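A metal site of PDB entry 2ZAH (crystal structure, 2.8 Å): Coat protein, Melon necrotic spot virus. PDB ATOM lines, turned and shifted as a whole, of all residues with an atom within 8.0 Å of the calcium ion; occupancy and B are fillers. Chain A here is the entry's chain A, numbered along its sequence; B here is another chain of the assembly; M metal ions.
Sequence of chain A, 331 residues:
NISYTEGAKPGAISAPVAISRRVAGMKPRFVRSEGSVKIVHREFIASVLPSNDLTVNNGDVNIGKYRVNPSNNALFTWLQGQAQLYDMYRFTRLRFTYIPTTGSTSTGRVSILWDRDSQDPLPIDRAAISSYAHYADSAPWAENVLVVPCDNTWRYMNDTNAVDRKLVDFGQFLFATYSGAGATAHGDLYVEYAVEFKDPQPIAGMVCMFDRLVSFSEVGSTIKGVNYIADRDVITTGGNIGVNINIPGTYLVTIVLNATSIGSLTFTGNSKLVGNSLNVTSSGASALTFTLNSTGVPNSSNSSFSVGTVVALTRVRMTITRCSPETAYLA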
ATOM      1  N   GLN A  84      -1.147  26.805  12.768  1.00  0.00           N
ATOM      2  CA  GLN A  84      -0.454  25.782  12.009  1.00  0.00           C
ATOM      3  C   GLN A  84       0.129  26.310  10.713  1.00  0.00           C
ATOM      4  O   GLN A  84       0.963  25.632  10.099  1.00  0.00           O
ATOM      5  CB  GLN A  84      -1.391  24.632  11.692  1.00  0.00           C
ATOM      6  CG  GLN A  84      -2.742  25.097  11.209  1.00  0.00           C
ATOM      7  CD  GLN A  84      -3.420  24.095  10.311  1.00  0.00           C
ATOM      8  OE1 GLN A  84      -2.805  23.111   9.881  1.00  0.00           O
ATOM      9  NE2 GLN A  84      -4.687  24.341   9.985  1.00  0.00           N
ATOM     10  N   LEU A  85      -0.279  27.507  10.297  1.00  0.00           N
ATOM     11  CA  LEU A  85       0.149  28.080   9.024  1.00  0.00           C
ATOM     12  C   LEU A  85       1.351  29.036   9.101  1.00  0.00           C
ATOM     13  O   LEU A  85       1.865  29.510   8.071  1.00  0.00           O
ATOM     14  CB  LEU A  85      -1.032  28.784   8.351  1.00  0.00           C
ATOM     15  CG  LEU A  85      -1.941  27.960   7.450  1.00  0.00           C
ATOM     16  CD1 LEU A  85      -2.581  26.815   8.185  1.00  0.00           C
ATOM     17  CD2 LEU A  85      -3.025  28.843   6.870  1.00  0.00           C
ATOM     18  N   TYR A  86       1.789  29.321  10.325  1.00  0.00           N
ATOM     19  CA  TYR A  86       2.810  30.335  10.550  1.00  0.00           C
ATOM     20  C   TYR A  86       3.937  29.832  11.433  1.00  0.00           C
ATOM     21  O   TYR A  86       3.755  28.874  12.176  1.00  0.00           O
ATOM     22  CB  TYR A  86       2.162  31.598  11.161  1.00  0.00           C
ATOM     23  CG  TYR A  86       1.237  32.302  10.196  1.00  0.00           C
ATOM     24  CD1 TYR A  86       1.705  33.311   9.352  1.00  0.00           C
ATOM     25  CD2 TYR A  86      -0.102  31.925  10.100  1.00  0.00           C
ATOM     26  CE1 TYR A  86       0.857  33.939   8.434  1.00  0.00           C
ATOM     27  CE2 TYR A  86      -0.964  32.551   9.178  1.00  0.00           C
ATOM     28  CZ  TYR A  86      -0.481  33.546   8.364  1.00  0.00           C
ATOM     29  OH  TYR A  86      -1.336  34.159   7.477  1.00  0.00           O
ATOM     30  N   ASP A  87       5.084  30.498  11.353  1.00  0.00           N
ATOM     31  CA  ASP A  87       6.264  30.107  12.114  1.00  0.00           C
ATOM     32  C   ASP A  87       6.407  30.748  13.486  1.00  0.00           C
ATOM     33  O   ASP A  87       6.928  30.118  14.400  1.00  0.00           O
ATOM     34  CB  ASP A  87       7.513  30.425  11.328  1.00  0.00           C
ATOM     35  CG  ASP A  87       8.179  29.180  10.796  1.00  0.00           C
ATOM     36  OD1 ASP A  87       8.398  29.059   9.552  1.00  0.00           O
ATOM     37  OD2 ASP A  87       8.475  28.284  11.635  1.00  0.00           O
ATOM     38  N   MET A  88       5.963  32.001  13.616  1.00  0.00           N
ATOM     39  CA  MET A  88       6.261  32.782  14.818  1.00  0.00           C
ATOM     40  C   MET A  88       5.080  33.592  15.292  1.00  0.00           C
ATOM     41  O   MET A  88       4.236  33.981  14.509  1.00  0.00           O
ATOM     42  CB  MET A  88       7.446  33.715  14.576  1.00  0.00           C
ATOM     43  CG  MET A  88       8.694  33.036  14.072  1.00  0.00           C
ATOM     44  SD  MET A  88      10.142  33.512  15.042  1.00  0.00           S
ATOM     45  CE  MET A  88      10.421  35.223  14.554  1.00  0.00           C
ATOM     46  N   TYR A 156       8.923  31.178  18.673  1.00  0.00           N
ATOM     47  CA  TYR A 156       8.660  30.136  17.687  1.00  0.00           C
ATOM     48  C   TYR A 156       7.412  29.354  18.040  1.00  0.00           C
ATOM     49  O   TYR A 156       7.229  28.902  19.170  1.00  0.00           O
ATOM     50  CB  TYR A 156       9.845  29.187  17.541  1.00  0.00           C
ATOM     51  CG  TYR A 156      11.048  29.838  16.908  1.00  0.00           C
ATOM     52  CD1 TYR A 156      12.101  30.293  17.696  1.00  0.00           C
ATOM     53  CD2 TYR A 156      11.120  30.009  15.533  1.00  0.00           C
ATOM     54  CE1 TYR A 156      13.209  30.898  17.123  1.00  0.00           C
ATOM     55  CE2 TYR A 156      12.202  30.601  14.953  1.00  0.00           C
ATOM     56  CZ  TYR A 156      13.250  31.058  15.755  1.00  0.00           C
ATOM     57  OH  TYR A 156      14.350  31.654  15.188  1.00  0.00           O
ATOM     58  N   ASN A 158       6.133  26.511  16.114  1.00  0.00           N
ATOM     59  CA  ASN A 158       6.191  25.076  15.766  1.00  0.00           C
ATOM     60  C   ASN A 158       6.557  24.202  16.943  1.00  0.00           C
ATOM     61  O   ASN A 158       7.462  24.524  17.735  1.00  0.00           O
ATOM     62  CB  ASN A 158       7.184  24.794  14.622  1.00  0.00           C
ATOM     63  CG  ASN A 158       6.805  25.490  13.321  1.00  0.00           C
ATOM     64  OD1 ASN A 158       5.672  25.363  12.818  1.00  0.00           O
ATOM     65  ND2 ASN A 158       7.748  26.231  12.766  1.00  0.00           N
ATOM     66  N   ASP A 199       5.561  34.159   9.916  1.00  0.00           N
ATOM     67  CA  ASP A 199       6.006  33.593   8.615  1.00  0.00           C
ATOM     68  C   ASP A 199       5.135  32.465   8.075  1.00  0.00           C
ATOM     69  O   ASP A 199       5.144  31.369   8.626  1.00  0.00           O
ATOM     70  CB  ASP A 199       7.455  33.111   8.673  1.00  0.00           C
ATOM     71  CG  ASP A 199       8.453  34.238   8.492  1.00  0.00           C
ATOM     72  OD1 ASP A 199       8.064  35.373   8.116  1.00  0.00           O
ATOM     73  OD2 ASP A 199       9.657  33.981   8.738  1.00  0.00           O
ATOM     74  N   PRO A 200       4.381  32.728   6.988  1.00  0.00           N
ATOM     75  CA  PRO A 200       3.673  31.631   6.346  1.00  0.00           C
ATOM     76  C   PRO A 200       4.602  30.458   6.086  1.00  0.00           C
ATOM     77  O   PRO A 200       5.782  30.650   5.768  1.00  0.00           O
ATOM     78  CB  PRO A 200       3.192  32.245   5.025  1.00  0.00           C
ATOM     79  CG  PRO A 200       3.013  33.668   5.357  1.00  0.00           C
ATOM     80  CD  PRO A 200       4.125  34.017   6.312  1.00  0.00           C
ATOM     81  N   GLN A 201       4.075  29.253   6.272  1.00  0.00           N
ATOM     82  CA  GLN A 201       4.871  28.027   6.151  1.00  0.00           C
ATOM     83  C   GLN A 201       3.955  26.872   5.698  1.00  0.00           C
ATOM     84  O   GLN A 201       2.726  27.027   5.719  1.00  0.00           O
ATOM     85  CB  GLN A 201       5.518  27.695   7.493  1.00  0.00           C
ATOM     86  CG  GLN A 201       4.504  27.403   8.587  1.00  0.00           C
ATOM     87  CD  GLN A 201       5.072  26.668   9.778  1.00  0.00           C
ATOM     88  OE1 GLN A 201       6.249  26.828  10.123  1.00  0.00           O
ATOM     89  NE2 GLN A 201       4.233  25.862  10.432  1.00  0.00           N
ATOM     90  N   PRO A 202       4.540  25.721   5.311  1.00  0.00           N
ATOM     91  CA  PRO A 202       3.714  24.545   5.081  1.00  0.00           C
ATOM     92  C   PRO A 202       2.914  24.229   6.336  1.00  0.00           C
ATOM     93  O   PRO A 202       3.449  24.325   7.451  1.00  0.00           O
ATOM     94  CB  PRO A 202       4.739  23.430   4.874  1.00  0.00           C
ATOM     95  CG  PRO A 202       5.935  24.092   4.448  1.00  0.00           C
ATOM     96  CD  PRO A 202       5.963  25.436   5.083  1.00  0.00           C
ATOM     97  N   ILE A 203       1.650  23.863   6.164  1.00  0.00           N
ATOM     98  CA  ILE A 203       0.771  23.640   7.299  1.00  0.00           C
ATOM     99  C   ILE A 203       1.274  22.542   8.229  1.00  0.00           C
ATOM    100  O   ILE A 203       1.727  21.481   7.774  1.00  0.00           O
ATOM    101  CB  ILE A 203      -0.688  23.373   6.871  1.00  0.00           C
ATOM    102  CG1 ILE A 203      -0.894  21.924   6.444  1.00  0.00           C
ATOM    103  CG2 ILE A 203      -1.108  24.324   5.738  1.00  0.00           C
ATOM    104  CD1 ILE A 203      -2.303  21.469   6.747  1.00  0.00           C
ATOM    105  N   TRP B 114      13.951  29.223   2.503  1.00  0.00           N
ATOM    106  CA  TRP B 114      14.473  29.482   3.828  1.00  0.00           C
ATOM    107  C   TRP B 114      13.355  29.456   4.856  1.00  0.00           C
ATOM    108  O   TRP B 114      12.335  30.142   4.702  1.00  0.00           O
ATOM    109  CB  TRP B 114      15.179  30.817   3.876  1.00  0.00           C
ATOM    110  CG  TRP B 114      15.799  31.152   5.190  1.00  0.00           C
ATOM    111  CD1 TRP B 114      17.004  30.728   5.669  1.00  0.00           C
ATOM    112  CD2 TRP B 114      15.254  32.018   6.185  1.00  0.00           C
ATOM    113  NE1 TRP B 114      17.241  31.266   6.903  1.00  0.00           N
ATOM    114  CE2 TRP B 114      16.184  32.078   7.244  1.00  0.00           C
ATOM    115  CE3 TRP B 114      14.072  32.764   6.284  1.00  0.00           C
ATOM    116  CZ2 TRP B 114      15.971  32.844   8.391  1.00  0.00           C
ATOM    117  CZ3 TRP B 114      13.855  33.528   7.423  1.00  0.00           C
ATOM    118  CH2 TRP B 114      14.795  33.564   8.459  1.00  0.00           C
ATOM    119  N   ASP B 115      13.570  28.669   5.906  1.00  0.00           N
ATOM    120  CA  ASP B 115      12.614  28.448   6.978  1.00  0.00           C
ATOM    121  C   ASP B 115      13.201  29.065   8.231  1.00  0.00           C
ATOM    122  O   ASP B 115      14.290  28.683   8.657  1.00  0.00           O
ATOM    123  CB  ASP B 115      12.439  26.927   7.149  1.00  0.00           C
ATOM    124  CG  ASP B 115      11.322  26.546   8.134  1.00  0.00           C
ATOM    125  OD1 ASP B 115      10.846  25.391   8.041  1.00  0.00           O
ATOM    126  OD2 ASP B 115      10.930  27.374   8.991  1.00  0.00           O
ATOM    127  N   ARG B 116      12.497  30.013   8.818  1.00  0.00           N
ATOM    128  CA  ARG B 116      13.005  30.732   9.997  1.00  0.00           C
ATOM    129  C   ARG B 116      13.288  29.824  11.190  1.00  0.00           C
ATOM    130  O   ARG B 116      14.090  30.166  12.064  1.00  0.00           O
ATOM    131  CB  ARG B 116      12.011  31.818  10.402  1.00  0.00           C
ATOM    132  CG  ARG B 116      12.570  32.868  11.327  1.00  0.00           C
ATOM    133  CD  ARG B 116      11.653  34.060  11.369  1.00  0.00           C
ATOM    134  NE  ARG B 116      12.426  35.296  11.199  1.00  0.00           N
ATOM    135  CZ  ARG B 116      12.362  36.101  10.136  1.00  0.00           C
ATOM    136  NH1 ARG B 116      11.540  35.834   9.128  1.00  0.00           N
ATOM    137  NH2 ARG B 116      13.105  37.187  10.097  1.00  0.00           N
ATOM    138  N   ASP B 117      12.615  28.680  11.218  1.00  0.00           N
ATOM    139  CA  ASP B 117      12.795  27.687  12.277  1.00  0.00           C
ATOM    140  C   ASP B 117      13.704  26.576  11.773  1.00  0.00           C
ATOM    141  O   ASP B 117      13.328  25.820  10.879  1.00  0.00           O
ATOM    142  CB  ASP B 117      11.425  27.138  12.662  1.00  0.00           C
ATOM    143  CG  ASP B 117      11.470  26.247  13.870  1.00  0.00           C
ATOM    144  OD1 ASP B 117      12.459  25.490  14.034  1.00  0.00           O
ATOM    145  OD2 ASP B 117      10.501  26.286  14.657  1.00  0.00           O
ATOM    146  N   SER B 118      14.906  26.471  12.316  1.00  0.00           N
ATOM    147  CA  SER B 118      15.872  25.511  11.781  1.00  0.00           C
ATOM    148  C   SER B 118      15.592  24.064  12.207  1.00  0.00           C
ATOM    149  O   SER B 118      16.296  23.151  11.795  1.00  0.00           O
ATOM    150  CB  SER B 118      17.282  25.890  12.174  1.00  0.00           C
ATOM    151  OG  SER B 118      17.479  25.718  13.548  1.00  0.00           O
ATOM    152  N   GLN B 119      14.572  23.869  13.018  1.00  0.00           N
ATOM    153  CA  GLN B 119      14.241  22.535  13.466  1.00  0.00           C
ATOM    154  C   GLN B 119      12.982  21.971  12.810  1.00  0.00           C
ATOM    155  O   GLN B 119      12.604  20.830  13.065  1.00  0.00           O
ATOM    156  CB  GLN B 119      14.122  22.502  14.983  1.00  0.00           C
ATOM    157  CG  GLN B 119      15.455  22.349  15.700  1.00  0.00           C
ATOM    158  CD  GLN B 119      15.359  22.640  17.197  1.00  0.00           C
ATOM    159  OE1 GLN B 119      15.027  23.755  17.623  1.00  0.00           O
ATOM    160  NE2 GLN B 119      15.652  21.634  17.995  1.00  0.00           N
ATOM    161  N   ASP B 120      12.343  22.779  11.961  1.00  0.00           N
ATOM    162  CA  ASP B 120      11.160  22.347  11.223  1.00  0.00           C
ATOM    163  C   ASP B 120      11.417  21.159  10.302  1.00  0.00           C
ATOM    164  O   ASP B 120      12.478  21.051   9.702  1.00  0.00           O
ATOM    165  CB  ASP B 120      10.596  23.506  10.414  1.00  0.00           C
ATOM    166  CG  ASP B 120       9.439  24.206  11.097  1.00  0.00           C
ATOM    167  OD1 ASP B 120       8.960  25.239  10.550  1.00  0.00           O
ATOM    168  OD2 ASP B 120       8.992  23.745  12.170  1.00  0.00           O
ATOM    169  N   PRO B 121      10.421  20.265  10.162  1.00  0.00           N
ATOM    170  CA  PRO B 121      10.596  19.062   9.343  1.00  0.00           C
ATOM    171  C   PRO B 121      10.731  19.414   7.882  1.00  0.00           C
ATOM    172  O   PRO B 121      10.287  20.476   7.470  1.00  0.00           O
ATOM    173  CB  PRO B 121       9.292  18.290   9.563  1.00  0.00           C
ATOM    174  CG  PRO B 121       8.711  18.878  10.815  1.00  0.00           C
ATOM    175  CD  PRO B 121       9.071  20.326  10.726  1.00  0.00           C
ATOM    176  N   SER B 131       4.680  27.013  -0.255  1.00  0.00           N
ATOM    177  CA  SER B 131       4.019  27.808   0.783  1.00  0.00           C
ATOM    178  C   SER B 131       4.954  28.524   1.742  1.00  0.00           C
ATOM    179  O   SER B 131       4.492  29.265   2.598  1.00  0.00           O
ATOM    180  CB  SER B 131       3.043  26.947   1.567  1.00  0.00           C
ATOM    181  OG  SER B 131       1.850  26.801   0.836  1.00  0.00           O
ATOM    182  N   TYR B 132       6.262  28.298   1.594  1.00  0.00           N
ATOM    183  CA  TYR B 132       7.231  29.020   2.420  1.00  0.00           C
ATOM    184  C   TYR B 132       7.173  30.506   2.101  1.00  0.00           C
ATOM    185  O   TYR B 132       7.099  30.892   0.935  1.00  0.00           O
ATOM    186  CB  TYR B 132       8.646  28.505   2.170  1.00  0.00           C
ATOM    187  CG  TYR B 132       8.918  27.157   2.748  1.00  0.00           C
ATOM    188  CD1 TYR B 132       9.491  27.027   4.000  1.00  0.00           C
ATOM    189  CD2 TYR B 132       8.573  25.983   2.052  1.00  0.00           C
ATOM    190  CE1 TYR B 132       9.734  25.776   4.559  1.00  0.00           C
ATOM    191  CE2 TYR B 132       8.825  24.731   2.607  1.00  0.00           C
ATOM    192  CZ  TYR B 132       9.396  24.640   3.851  1.00  0.00           C
ATOM    193  OH  TYR B 132       9.645  23.432   4.420  1.00  0.00           O
ATOM    194  N   ALA B 133       7.195  31.346   3.133  1.00  0.00           N
ATOM    195  CA  ALA B 133       7.218  32.790   2.932  1.00  0.00           C
ATOM    196  C   ALA B 133       8.443  33.202   2.114  1.00  0.00           C
ATOM    197  O   ALA B 133       8.320  33.978   1.180  1.00  0.00           O
ATOM    198  CB  ALA B 133       7.180  33.524   4.272  1.00  0.00           C
ATOM    199  N   GLN B 172      16.958  27.853   8.595  1.00  0.00           N
ATOM    200  CA  GLN B 172      17.650  26.887   7.765  1.00  0.00           C
ATOM    201  C   GLN B 172      17.379  27.150   6.304  1.00  0.00           C
ATOM    202  O   GLN B 172      16.240  27.400   5.900  1.00  0.00           O
ATOM    203  CB  GLN B 172      17.230  25.460   8.133  1.00  0.00           C
ATOM    204  CG  GLN B 172      15.762  25.162   7.911  1.00  0.00           C
ATOM    205  CD  GLN B 172      15.427  23.733   8.292  1.00  0.00           C
ATOM    206  OE1 GLN B 172      16.148  22.796   7.958  1.00  0.00           O
ATOM    207  NE2 GLN B 172      14.315  23.563   9.007  1.00  0.00           N
ATOM    208  N   LEU B 174      17.127  25.472   2.635  1.00  0.00           N
ATOM    209  CA  LEU B 174      16.832  24.169   2.047  1.00  0.00           C
ATOM    210  C   LEU B 174      16.431  24.364   0.600  1.00  0.00           C
ATOM    211  O   LEU B 174      15.992  25.433   0.219  1.00  0.00           O
ATOM    212  CB  LEU B 174      15.756  23.407   2.848  1.00  0.00           C
ATOM    213  CG  LEU B 174      14.336  23.945   2.912  1.00  0.00           C
ATOM    214  CD1 LEU B 174      13.424  22.860   3.371  1.00  0.00           C
ATOM    215  CD2 LEU B 174      14.249  25.135   3.837  1.00  0.00           C
HETATM  216 CA    CA M   1       8.486  26.670   8.815  1.00  0.00          CA
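The calcium ion is bound by the side-chain carboxylate (OD1) of Asp 120 of chain B, the side-chain carboxylate (OD1) of Asp 87, the side-chain carboxylate (OD2) of Asp 115 of chain B, the side-chain amide oxygen (OE1) of Gln 201 and the side-chain carboxylate (OD1) of Asp 115 of chain B.
Within 4 Å of the calcium ion: Asp 87, Gln 201, Asp 115 of chain B and Asp 120 of chain B.
O of Asp 115 of chain B sits at hydrogen-bond distance from N of Gln 172 of chain B.
The side-chain carboxylate (OD2) of Asp 115 of chain B lies close to the backbone NH (N) of Asp 117 of chain B.
The backbone NH of Asp 87 sits at hydrogen-bond distance from the backbone carbonyl oxygen of Asp 199 (2.9 Å).
N of Asp 120 of chain B lies within hydrogen-bond range of OD1 of Asp 117 of chain B (3.4 Å).
The backbone carbonyl oxygen (O) of Asp 120 of chain B sits at hydrogen-bond distance from the side-chain amide nitrogen (NE2) of Gln 172 of chain B, at 3.2 Å.
The side-chain carboxylate (OD2) of Asp 87 sits at hydrogen-bond distance from the side-chain amide nitrogen (ND2) of Asn 158 (2.5 Å).
O of Leu 85 lies within hydrogen-bond range of N of Gln 201, at 2.9 Å.
NE2 of Gln 201 sits at hydrogen-bond distance from O of Gln 84 (3.3 Å).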
